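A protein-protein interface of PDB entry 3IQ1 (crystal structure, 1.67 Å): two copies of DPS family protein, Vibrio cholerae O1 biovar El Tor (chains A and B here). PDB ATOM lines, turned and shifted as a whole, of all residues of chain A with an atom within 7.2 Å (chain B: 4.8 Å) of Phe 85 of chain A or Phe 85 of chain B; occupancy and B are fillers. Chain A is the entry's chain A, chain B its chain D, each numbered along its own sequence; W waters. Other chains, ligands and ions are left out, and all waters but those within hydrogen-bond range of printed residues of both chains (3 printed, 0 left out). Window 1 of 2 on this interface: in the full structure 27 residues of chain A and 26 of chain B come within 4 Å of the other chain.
Met 35 of chain A touches Tyr 88 of chain B, and with the chains exchanged Tyr 88 of chain A touches Met 35 of chain B.
Phe 85 of chain A touches its own counterpart, Phe 85 of chain B.
Phe 85 of chain A touches Glu 96 of chain B, and with the chains exchanged Glu 96 of chain A touches Phe 85 of chain B.
Ser 86 of chain A touches Leu 89 of chain B, and with the chains exchanged Leu 89 of chain A touches Ser 86 of chain B.
Positions printed for both chains: 31, 32, 35, 83, 84, 85, 86, 87, 88, 89 and 96.
Of the 22 pairs that touch across the chains among the printed residues, 19 have their exchanged pair printed and touching as well.
Among the printed residues, merely in contact across the chains: Phe 85 of chain A with Phe 85 of chain B (3.3 Å), Thr 98 of chain A with His 83 of chain B (3.4 Å), Phe 85 of chain A with Gln 31 of chain B (3.4 Å), Ser 84 of chain A with Glu 96 of chain B (3.4 Å), Met 35 of chain A with Tyr 88 of chain B (3.5 Å), Glu 96 of chain A with Ser 84 of chain B (3.5 Å), Gln 31 of chain A with Phe 85 of chain B (3.5 Å), Tyr 88 of chain A with Met 35 of chain B (3.7 Å), His 83 of chain A with Met 35 of chain B (3.7 Å), Met 35 of chain A with His 83 of chain B (3.7 Å), Met 35 of chain A with Phe 85 of chain B (3.8 Å), Phe 85 of chain A with Leu 89 of chain B (3.8 Å), Thr 98 of chain A with Ser 84 of chain B (3.8 Å), Leu 89 of chain A with Phe 85 of chain B (3.9 Å), Phe 85 of chain A with Met 35 of chain B (3.9 Å), Ser 86 of chain A with Leu 89 of chain B (3.9 Å), Leu 89 of chain A with Ser 86 of chain B (3.9 Å) and Val 32 of chain A with Phe 85 of chain B (3.98 Å).
Phe 85 of chain A touches just these residues of chain B: Gln 31, Met 35, Phe 85, Leu 89 and Glu 96.
Of chain A, only Gln 31 (3.5 Å), Val 32 (3.98 Å), Met 35 (3.8 Å), Phe 85 (3.3 Å), Leu 89 (3.9 Å) and Glu 96 (3.2 Å) come within 4 Å of Phe 85 of chain B.
Of the printed residues of chain A, Ser 84 of chain B touches Glu 96 and Thr 98.
Printed residues of chain B within 4 Å of Ser 84 of chain A: Glu 96.
Printed residues of chain B within 4 Å of Val 32 of chain A: Phe 85 (3.98 Å).
Of the printed residues of chain B, Ser 86 of chain A touches Leu 89 and Glu 96.
The nearest printed residue of chain B that does not touch Phe 85 of chain A is Val 32 of chain B (4.1 Å).
Of the 11 printed residues of chain B, 9 touch a printed residue of chain A.
Hydrophobic or aromatic side chains of chain B that line the printed part of chain A: Met 35, His 83, Phe 85, Tyr 88 and Leu 89.
Printed residues of chain A that touch a printed residue of chain B: Gln 31, Val 32, Met 35, His 83, Ser 84, Phe 85, Ser 86, Tyr 88, Leu 89, Glu 96 and Thr 98.
Hydrophobic or aromatic side chains of chain A that line the printed part of chain B: Met 35, Phe 85, Tyr 88 and Leu 89.
Along chain A the printed residues that touch a printed residue of chain B span positions 31 to 98.
Among the printed residues, 22 pairs touch across the chains.
N of Phe 85 of chain A is in hydrogen-bond range of OE2 of Glu 96 of chain B, 3.3 Å away.
OG of Ser 86 of chain A is in hydrogen-bond range of OE1 of Glu 96 of chain B (2.7 Å).
The side-chain carboxylate (OE2) of Glu 96 of chain A lies within hydrogen-bond range of the backbone NH (N) of Phe 85 of chain B (3.2 Å).
OE1 of Glu 96 of chain A lies within hydrogen-bond range of OG of Ser 86 of chain B (2.8 Å).
NE2 of Gln 31 of chain A lies within hydrogen-bond range of OH of Tyr 88 of chain A (3.1 Å).
The backbone carbonyl oxygen of Val 32 of chain A lies close to the side-chain amide oxygen of Asn 36 of chain A (3.5 Å).
The side-chain hydroxyl (OH) of Tyr 88 of chain A lies within hydrogen-bond range of the backbone carbonyl oxygen (O) of Met 82 of chain A (2.7 Å).
OG of Ser 84 of chain A sits at hydrogen-bond distance from N of Gly 87 of chain A (3.1 Å).
NE2 of Gln 31 of chain B lies within hydrogen-bond range of OH of Tyr 88 of chain B.
OG of Ser 84 of chain B sits at hydrogen-bond distance from N of Gly 87 of chain B (3.1 Å).
Water W3 bridges the side-chain carboxylate of Glu 96 of chain B (2.7 Å) and the backbone NH of Phe 85 of chain A (2.8 Å).
Water W1 bridges the backbone NH (N) of Phe 85 of chain B and the side-chain carboxylate (OE2) of Glu 96 of chain A.
Water W2 lies within hydrogen-bond range of the backbone carbonyl oxygen of His 83 of chain B (2.8 Å) and the side-chain amide oxygen of Asn 36 of chain A (2.9 Å).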
ATOM      1  N   ALA A  28      27.095  -3.723  31.643  1.00  0.00           N
ATOM      2  CA  ALA A  28      26.442  -4.051  30.375  1.00  0.00           C
ATOM      3  C   ALA A  28      27.463  -4.642  29.438  1.00  0.00           C
ATOM      4  O   ALA A  28      27.183  -5.634  28.706  1.00  0.00           O
ATOM      5  CB  ALA A  28      25.818  -2.842  29.744  1.00  0.00           C
ATOM      6  N   TYR A  30      30.357  -6.121  30.313  1.00  0.00           N
ATOM      7  CA  TYR A  30      30.714  -7.457  30.779  1.00  0.00           C
ATOM      8  C   TYR A  30      29.695  -8.502  30.365  1.00  0.00           C
ATOM      9  O   TYR A  30      30.058  -9.642  30.060  1.00  0.00           O
ATOM     10  CB  TYR A  30      30.808  -7.487  32.308  1.00  0.00           C
ATOM     11  CG  TYR A  30      32.161  -7.235  32.876  1.00  0.00           C
ATOM     12  CD1 TYR A  30      32.601  -5.985  33.121  1.00  0.00           C
ATOM     13  CD2 TYR A  30      33.012  -8.286  33.147  1.00  0.00           C
ATOM     14  CE1 TYR A  30      33.877  -5.774  33.661  1.00  0.00           C
ATOM     15  CE2 TYR A  30      34.297  -8.085  33.658  1.00  0.00           C
ATOM     16  CZ  TYR A  30      34.726  -6.827  33.886  1.00  0.00           C
ATOM     17  OH  TYR A  30      36.007  -6.617  34.404  1.00  0.00           O
ATOM     18  N   GLN A  31      28.419  -8.160  30.453  1.00  0.00           N
ATOM     19  CA  GLN A  31      27.369  -9.143  30.208  1.00  0.00           C
ATOM     20  C   GLN A  31      27.347  -9.569  28.721  1.00  0.00           C
ATOM     21  O   GLN A  31      27.367 -10.774  28.409  1.00  0.00           O
ATOM     22  CB  GLN A  31      26.018  -8.576  30.656  1.00  0.00           C
ATOM     23  CG  GLN A  31      25.819  -8.527  32.165  1.00  0.00           C
ATOM     24  CD  GLN A  31      25.412  -9.867  32.754  1.00  0.00           C
ATOM     25  OE1 GLN A  31      25.788 -10.896  32.222  1.00  0.00           O
ATOM     26  NE2 GLN A  31      24.662  -9.869  33.848  1.00  0.00           N
ATOM     27  N   VAL A  32      27.458  -8.597  27.806  1.00  0.00           N
ATOM     28  CA  VAL A  32      27.523  -8.916  26.372  1.00  0.00           C
ATOM     29  C   VAL A  32      28.797  -9.700  26.063  1.00  0.00           C
ATOM     30  O   VAL A  32      28.763 -10.682  25.325  1.00  0.00           O
ATOM     31  CB  VAL A  32      27.343  -7.694  25.464  1.00  0.00           C
ATOM     32  CG1 VAL A  32      27.520  -8.069  23.994  1.00  0.00           C
ATOM     33  CG2 VAL A  32      25.967  -7.041  25.674  1.00  0.00           C
ATOM     34  N   PHE A  33      29.901  -9.303  26.685  1.00  0.00           N
ATOM     35  CA  PHE A  33      31.164 -10.000  26.509  1.00  0.00           C
ATOM     36  C   PHE A  33      31.150 -11.433  27.016  1.00  0.00           C
ATOM     37  O   PHE A  33      31.673 -12.327  26.355  1.00  0.00           O
ATOM     38  CB  PHE A  33      32.210  -9.195  27.190  1.00  0.00           C
ATOM     39  CG  PHE A  33      33.635  -9.580  26.880  1.00  0.00           C
ATOM     40  CD1 PHE A  33      34.096  -9.681  25.572  1.00  0.00           C
ATOM     41  CD2 PHE A  33      34.529  -9.668  27.897  1.00  0.00           C
ATOM     42  CE1 PHE A  33      35.431  -9.957  25.305  1.00  0.00           C
ATOM     43  CE2 PHE A  33      35.871  -9.938  27.627  1.00  0.00           C
ATOM     44  CZ  PHE A  33      36.320 -10.033  26.362  1.00  0.00           C
ATOM     45  N   TYR A  34      30.564 -11.648  28.178  1.00  0.00           N
ATOM     46  CA  TYR A  34      30.394 -12.971  28.717  1.00  0.00           C
ATOM     47  C   TYR A  34      29.606 -13.838  27.718  1.00  0.00           C
ATOM     48  O   TYR A  34      29.987 -14.979  27.468  1.00  0.00           O
ATOM     49  CB  TYR A  34      29.683 -12.873  30.064  1.00  0.00           C
ATOM     50  CG  TYR A  34      29.202 -14.216  30.576  1.00  0.00           C
ATOM     51  CD1 TYR A  34      30.034 -15.014  31.361  1.00  0.00           C
ATOM     52  CD2 TYR A  34      27.929 -14.674  30.313  1.00  0.00           C
ATOM     53  CE1 TYR A  34      29.619 -16.211  31.860  1.00  0.00           C
ATOM     54  CE2 TYR A  34      27.493 -15.901  30.836  1.00  0.00           C
ATOM     55  CZ  TYR A  34      28.360 -16.667  31.579  1.00  0.00           C
ATOM     56  OH  TYR A  34      27.987 -17.897  32.078  1.00  0.00           O
ATOM     57  N   MET A  35      28.508 -13.307  27.191  1.00  0.00           N
ATOM     58  CA  MET A  35      27.676 -14.054  26.269  1.00  0.00           C
ATOM     59  C   MET A  35      28.462 -14.438  25.025  1.00  0.00           C
ATOM     60  O   MET A  35      28.418 -15.581  24.562  1.00  0.00           O
ATOM     61  CB  MET A  35      26.397 -13.266  25.885  1.00  0.00           C
ATOM     62  CG  MET A  35      25.403 -13.976  25.076  1.00  0.00           C
ATOM     63  SD  MET A  35      24.611 -15.408  26.155  1.00  0.00           S
ATOM     64  CE  MET A  35      25.322 -16.917  25.216  1.00  0.00           C
ATOM     65  N   ASN A  36      29.249 -13.480  24.517  1.00  0.00           N
ATOM     66  CA  ASN A  36      30.076 -13.729  23.374  1.00  0.00           C
ATOM     67  C   ASN A  36      31.082 -14.859  23.674  1.00  0.00           C
ATOM     68  O   ASN A  36      31.319 -15.774  22.870  1.00  0.00           O
ATOM     69  CB  ASN A  36      30.860 -12.460  23.004  1.00  0.00           C
ATOM     70  CG  ASN A  36      30.020 -11.396  22.362  1.00  0.00           C
ATOM     71  OD1 ASN A  36      28.868 -11.635  21.993  1.00  0.00           O
ATOM     72  ND2 ASN A  36      30.608 -10.197  22.178  1.00  0.00           N
ATOM     73  N   MET A  82      21.681  -2.787  36.568  1.00  0.00           N
ATOM     74  CA  MET A  82      20.930  -3.258  35.417  1.00  0.00           C
ATOM     75  C   MET A  82      20.892  -4.796  35.496  1.00  0.00           C
ATOM     76  O   MET A  82      21.872  -5.431  35.858  1.00  0.00           O
ATOM     77  CB  MET A  82      21.592  -2.787  34.118  1.00  0.00           C
ATOM     78  CG  MET A  82      20.976  -1.590  33.533  1.00  0.00           C
ATOM     79  SD  MET A  82      21.841  -1.294  31.775  1.00  0.00           S
ATOM     80  CE  MET A  82      23.460  -0.771  32.424  1.00  0.00           C
ATOM     81  N   HIS A  83      19.757  -5.368  35.129  1.00  0.00           N
ATOM     82  CA  HIS A  83      19.518  -6.805  35.325  1.00  0.00           C
ATOM     83  C   HIS A  83      18.533  -7.383  34.302  1.00  0.00           C
ATOM     84  O   HIS A  83      17.735  -8.279  34.607  1.00  0.00           O
ATOM     85  CB  HIS A  83      19.146  -7.169  36.778  1.00  0.00           C
ATOM     86  CG  HIS A  83      17.907  -6.483  37.295  1.00  0.00           C
ATOM     87  ND1 HIS A  83      17.900  -5.155  37.677  1.00  0.00           N
ATOM     88  CD2 HIS A  83      16.659  -6.956  37.527  1.00  0.00           C
ATOM     89  CE1 HIS A  83      16.702  -4.845  38.155  1.00  0.00           C
ATOM     90  NE2 HIS A  83      15.923  -5.918  38.063  1.00  0.00           N
ATOM     91  N   SER A  84      18.628  -6.884  33.082  1.00  0.00           N
ATOM     92  CA  SER A  84      17.875  -7.467  31.955  1.00  0.00           C
ATOM     93  C   SER A  84      18.771  -7.421  30.707  1.00  0.00           C
ATOM     94  O   SER A  84      19.527  -6.464  30.523  1.00  0.00           O
ATOM     95  CB  SER A  84      16.603  -6.703  31.678  1.00  0.00           C
ATOM     96  OG  SER A  84      16.828  -5.358  31.324  1.00  0.00           O
ATOM     97  N   PHE A  85      18.645  -8.456  29.875  1.00  0.00           N
ATOM     98  CA  PHE A  85      19.265  -8.461  28.547  1.00  0.00           C
ATOM     99  C   PHE A  85      18.928  -7.202  27.723  1.00  0.00           C
ATOM    100  O   PHE A  85      19.775  -6.602  27.101  1.00  0.00           O
ATOM    101  CB  PHE A  85      18.733  -9.666  27.745  1.00  0.00           C
ATOM    102  CG  PHE A  85      19.143 -11.041  28.272  1.00  0.00           C
ATOM    103  CD1 PHE A  85      20.208 -11.234  29.162  1.00  0.00           C
ATOM    104  CD2 PHE A  85      18.510 -12.161  27.802  1.00  0.00           C
ATOM    105  CE1 PHE A  85      20.578 -12.501  29.601  1.00  0.00           C
ATOM    106  CE2 PHE A  85      18.904 -13.402  28.215  1.00  0.00           C
ATOM    107  CZ  PHE A  85      19.930 -13.579  29.123  1.00  0.00           C
ATOM    108  N   SER A  86      17.669  -6.763  27.761  1.00  0.00           N
ATOM    109  CA  SER A  86      17.302  -5.612  26.965  1.00  0.00           C
ATOM    110  C   SER A  86      18.006  -4.360  27.466  1.00  0.00           C
ATOM    111  O   SER A  86      18.425  -3.572  26.655  1.00  0.00           O
ATOM    112  CB  SER A  86      15.800  -5.430  26.904  1.00  0.00           C
ATOM    113  OG  SER A  86      15.278  -5.223  28.180  1.00  0.00           O
ATOM    114  N   GLY A  87      18.145  -4.196  28.780  1.00  0.00           N
ATOM    115  CA  GLY A  87      18.930  -3.085  29.316  1.00  0.00           C
ATOM    116  C   GLY A  87      20.375  -3.143  28.922  1.00  0.00           C
ATOM    117  O   GLY A  87      20.960  -2.158  28.474  1.00  0.00           O
ATOM    118  N   TYR A  88      20.968  -4.323  29.049  1.00  0.00           N
ATOM    119  CA  TYR A  88      22.361  -4.464  28.652  1.00  0.00           C
ATOM    120  C   TYR A  88      22.615  -4.135  27.183  1.00  0.00           C
ATOM    121  O   TYR A  88      23.618  -3.520  26.848  1.00  0.00           O
ATOM    122  CB  TYR A  88      22.897  -5.877  28.933  1.00  0.00           C
ATOM    123  CG  TYR A  88      22.843  -6.317  30.376  1.00  0.00           C
ATOM    124  CD1 TYR A  88      23.153  -5.440  31.386  1.00  0.00           C
ATOM    125  CD2 TYR A  88      22.494  -7.604  30.708  1.00  0.00           C
ATOM    126  CE1 TYR A  88      23.138  -5.811  32.722  1.00  0.00           C
ATOM    127  CE2 TYR A  88      22.471  -8.001  32.055  1.00  0.00           C
ATOM    128  CZ  TYR A  88      22.778  -7.089  33.049  1.00  0.00           C
ATOM    129  OH  TYR A  88      22.765  -7.523  34.353  1.00  0.00           O
ATOM    130  N   LEU A  89      21.733  -4.593  26.302  1.00  0.00           N
ATOM    131  CA  LEU A  89      21.931  -4.376  24.870  1.00  0.00           C
ATOM    132  C   LEU A  89      21.838  -2.895  24.532  1.00  0.00           C
ATOM    133  O   LEU A  89      22.554  -2.407  23.647  1.00  0.00           O
ATOM    134  CB  LEU A  89      20.942  -5.175  24.049  1.00  0.00           C
ATOM    135  CG  LEU A  89      21.185  -6.691  23.953  1.00  0.00           C
ATOM    136  CD1 LEU A  89      19.934  -7.356  23.224  1.00  0.00           C
ATOM    137  CD2 LEU A  89      22.518  -6.955  23.202  1.00  0.00           C
ATOM    138  N   LYS A  90      20.995  -2.165  25.240  1.00  0.00           N
ATOM    139  CA  LYS A  90      20.912  -0.716  25.040  1.00  0.00           C
ATOM    140  C   LYS A  90      22.167   0.030  25.462  1.00  0.00           C
ATOM    141  O   LYS A  90      22.539   1.039  24.838  1.00  0.00           O
ATOM    142  CB  LYS A  90      19.710  -0.165  25.783  1.00  0.00           C
ATOM    143  CG  LYS A  90      18.466  -0.272  24.966  1.00  0.00           C
ATOM    144  CD  LYS A  90      17.234   0.296  25.728  1.00  0.00           C
ATOM    145  CE  LYS A  90      16.259  -0.839  26.135  1.00  0.00           C
ATOM    146  NZ  LYS A  90      15.819  -0.707  27.557  1.00  0.00           N
ATOM    147  N   ALA A  91      22.790  -0.423  26.553  1.00  0.00           N
ATOM    148  CA  ALA A  91      23.919   0.265  27.164  1.00  0.00           C
ATOM    149  C   ALA A  91      25.310  -0.151  26.660  1.00  0.00           C
ATOM    150  O   ALA A  91      26.262   0.675  26.751  1.00  0.00           O
ATOM    151  CB  ALA A  91      23.895   0.103  28.685  1.00  0.00           C
ATOM    152  N   GLU A  96      27.316  -7.732  20.054  1.00  0.00           N
ATOM    153  CA  GLU A  96      27.082  -9.196  20.028  1.00  0.00           C
ATOM    154  C   GLU A  96      27.946  -9.828  18.924  1.00  0.00           C
ATOM    155  O   GLU A  96      27.995  -9.319  17.778  1.00  0.00           O
ATOM    156  CB  GLU A  96      25.617  -9.514  19.802  1.00  0.00           C
ATOM    157  CG  GLU A  96      24.663  -8.917  20.849  1.00  0.00           C
ATOM    158  CD  GLU A  96      23.277  -9.403  20.662  1.00  0.00           C
ATOM    159  OE1 GLU A  96      22.748  -9.151  19.558  1.00  0.00           O
ATOM    160  OE2 GLU A  96      22.724  -9.994  21.585  1.00  0.00           O
ATOM    161  N   THR A  98      28.468 -13.360  17.082  1.00  0.00           N
ATOM    162  CA  THR A  98      27.908 -14.710  16.894  1.00  0.00           C
ATOM    163  C   THR A  98      28.672 -15.436  15.812  1.00  0.00           C
ATOM    164  O   THR A  98      29.260 -14.804  14.921  1.00  0.00           O
ATOM    165  CB  THR A  98      26.428 -14.646  16.607  1.00  0.00           C
ATOM    166  OG1 THR A  98      26.207 -13.843  15.436  1.00  0.00           O
ATOM    167  CG2 THR A  98      25.639 -14.038  17.809  1.00  0.00           C
ATOM    168  N   GLN B  31      17.585 -18.947  29.543  1.00  0.00           N
ATOM    169  CA  GLN B  31      18.464 -17.791  29.625  1.00  0.00           C
ATOM    170  C   GLN B  31      17.762 -16.565  30.214  1.00  0.00           C
ATOM    171  O   GLN B  31      18.300 -15.878  31.064  1.00  0.00           O
ATOM    172  CB  GLN B  31      19.039 -17.511  28.251  1.00  0.00           C
ATOM    173  CG  GLN B  31      20.116 -18.510  27.766  1.00  0.00           C
ATOM    174  CD  GLN B  31      21.476 -18.220  28.322  1.00  0.00           C
ATOM    175  OE1 GLN B  31      21.583 -17.604  29.377  1.00  0.00           O
ATOM    176  NE2 GLN B  31      22.513 -18.614  27.630  1.00  0.00           N
ATOM    177  N   VAL B  32      16.530 -16.298  29.799  1.00  0.00           N
ATOM    178  CA  VAL B  32      15.776 -15.192  30.392  1.00  0.00           C
ATOM    179  C   VAL B  32      15.463 -15.497  31.848  1.00  0.00           C
ATOM    180  O   VAL B  32      15.556 -14.606  32.730  1.00  0.00           O
ATOM    181  CB  VAL B  32      14.492 -14.866  29.571  1.00  0.00           C
ATOM    182  CG1 VAL B  32      13.636 -13.786  30.239  1.00  0.00           C
ATOM    183  CG2 VAL B  32      14.882 -14.399  28.135  1.00  0.00           C
ATOM    184  N   MET B  35      18.505 -14.923  33.993  1.00  0.00           N
ATOM    185  CA  MET B  35      18.738 -13.476  34.180  1.00  0.00           C
ATOM    186  C   MET B  35      17.791 -12.944  35.229  1.00  0.00           C
ATOM    187  O   MET B  35      18.209 -12.212  36.108  1.00  0.00           O
ATOM    188  CB  MET B  35      18.486 -12.733  32.876  1.00  0.00           C
ATOM    189  CG  MET B  35      18.915 -11.292  32.861  1.00  0.00           C
ATOM    190  SD  MET B  35      20.873 -11.078  33.197  1.00  0.00           S
ATOM    191  CE  MET B  35      20.861 -10.621  34.889  1.00  0.00           C
ATOM    192  N   HIS B  83      22.983 -18.116  20.795  1.00  0.00           N
ATOM    193  CA  HIS B  83      24.049 -17.602  21.653  1.00  0.00           C
ATOM    194  C   HIS B  83      24.151 -16.081  21.669  1.00  0.00           C
ATOM    195  O   HIS B  83      25.219 -15.492  21.697  1.00  0.00           O
ATOM    196  CB  HIS B  83      25.374 -18.308  21.356  1.00  0.00           C
ATOM    197  CG  HIS B  83      25.853 -18.184  19.947  1.00  0.00           C
ATOM    198  ND1 HIS B  83      25.265 -18.883  18.908  1.00  0.00           N
ATOM    199  CD2 HIS B  83      26.843 -17.448  19.403  1.00  0.00           C
ATOM    200  CE1 HIS B  83      25.906 -18.598  17.788  1.00  0.00           C
ATOM    201  NE2 HIS B  83      26.873 -17.740  18.054  1.00  0.00           N
ATOM    202  N   SER B  84      22.993 -15.419  21.673  1.00  0.00           N
ATOM    203  CA  SER B  84      22.968 -13.958  21.798  1.00  0.00           C
ATOM    204  C   SER B  84      21.726 -13.576  22.569  1.00  0.00           C
ATOM    205  O   SER B  84      20.680 -14.242  22.432  1.00  0.00           O
ATOM    206  CB  SER B  84      22.949 -13.261  20.443  1.00  0.00           C
ATOM    207  OG  SER B  84      21.803 -13.587  19.653  1.00  0.00           O
ATOM    208  N   PHE B  85      21.850 -12.521  23.395  1.00  0.00           N
ATOM    209  CA  PHE B  85      20.713 -11.949  24.100  1.00  0.00           C
ATOM    210  C   PHE B  85      19.586 -11.608  23.126  1.00  0.00           C
ATOM    211  O   PHE B  85      18.423 -11.861  23.401  1.00  0.00           O
ATOM    212  CB  PHE B  85      21.140 -10.650  24.812  1.00  0.00           C
ATOM    213  CG  PHE B  85      22.142 -10.833  25.990  1.00  0.00           C
ATOM    214  CD1 PHE B  85      22.392 -12.072  26.607  1.00  0.00           C
ATOM    215  CD2 PHE B  85      22.801  -9.711  26.495  1.00  0.00           C
ATOM    216  CE1 PHE B  85      23.247 -12.184  27.661  1.00  0.00           C
ATOM    217  CE2 PHE B  85      23.689  -9.840  27.570  1.00  0.00           C
ATOM    218  CZ  PHE B  85      23.906 -11.072  28.163  1.00  0.00           C
ATOM    219  N   SER B  86      19.912 -11.013  21.983  1.00  0.00           N
ATOM    220  CA  SER B  86      18.837 -10.607  21.086  1.00  0.00           C
ATOM    221  C   SER B  86      18.085 -11.814  20.541  1.00  0.00           C
ATOM    222  O   SER B  86      16.856 -11.781  20.412  1.00  0.00           O
ATOM    223  CB  SER B  86      19.374  -9.704  19.982  1.00  0.00           C
ATOM    224  OG  SER B  86      20.304 -10.369  19.198  1.00  0.00           O
ATOM    225  N   GLY B  87      18.812 -12.869  20.255  1.00  0.00           N
ATOM    226  CA  GLY B  87      18.167 -14.125  19.841  1.00  0.00           C
ATOM    227  C   GLY B  87      17.279 -14.701  20.919  1.00  0.00           C
ATOM    228  O   GLY B  87      16.138 -15.067  20.663  1.00  0.00           O
ATOM    229  N   TYR B  88      17.761 -14.707  22.157  1.00  0.00           N
ATOM    230  CA  TYR B  88      16.960 -15.278  23.242  1.00  0.00           C
ATOM    231  C   TYR B  88      15.685 -14.485  23.470  1.00  0.00           C
ATOM    232  O   TYR B  88      14.626 -15.046  23.705  1.00  0.00           O
ATOM    233  CB  TYR B  88      17.753 -15.354  24.563  1.00  0.00           C
ATOM    234  CG  TYR B  88      18.980 -16.237  24.540  1.00  0.00           C
ATOM    235  CD1 TYR B  88      18.989 -17.464  23.903  1.00  0.00           C
ATOM    236  CD2 TYR B  88      20.148 -15.849  25.199  1.00  0.00           C
ATOM    237  CE1 TYR B  88      20.101 -18.254  23.894  1.00  0.00           C
ATOM    238  CE2 TYR B  88      21.267 -16.641  25.170  1.00  0.00           C
ATOM    239  CZ  TYR B  88      21.248 -17.834  24.530  1.00  0.00           C
ATOM    240  OH  TYR B  88      22.388 -18.630  24.545  1.00  0.00           O
ATOM    241  N   LEU B  89      15.778 -13.165  23.398  1.00  0.00           N
ATOM    242  CA  LEU B  89      14.626 -12.305  23.659  1.00  0.00           C
ATOM    243  C   LEU B  89      13.612 -12.512  22.558  1.00  0.00           C
ATOM    244  O   LEU B  89      12.421 -12.383  22.775  1.00  0.00           O
ATOM    245  CB  LEU B  89      15.042 -10.833  23.750  1.00  0.00           C
ATOM    246  CG  LEU B  89      15.769 -10.380  25.046  1.00  0.00           C
ATOM    247  CD1 LEU B  89      16.309  -8.922  24.871  1.00  0.00           C
ATOM    248  CD2 LEU B  89      14.864 -10.551  26.283  1.00  0.00           C
ATOM    249  N   GLU B  96      11.034 -10.971  30.648  1.00  0.00           N
ATOM    250  CA  GLU B  96      11.937 -10.312  31.604  1.00  0.00           C
ATOM    251  C   GLU B  96      11.168  -9.820  32.830  1.00  0.00           C
ATOM    252  O   GLU B  96      10.057  -9.264  32.708  1.00  0.00           O
ATOM    253  CB  GLU B  96      12.637  -9.135  30.933  1.00  0.00           C
ATOM    254  CG  GLU B  96      13.448  -9.531  29.712  1.00  0.00           C
ATOM    255  CD  GLU B  96      14.258  -8.374  29.157  1.00  0.00           C
ATOM    256  OE1 GLU B  96      13.654  -7.316  28.912  1.00  0.00           O
ATOM    257  OE2 GLU B  96      15.492  -8.509  28.965  1.00  0.00           O
HETATM  258  O   HOH W   1      24.307 -11.235  23.500  1.00  0.00           O
HETATM  259  O   HOH W   2      26.340 -12.936  21.642  1.00  0.00           O
HETATM  260  O   HOH W   3      16.723 -10.431  30.490  1.00  0.00           O
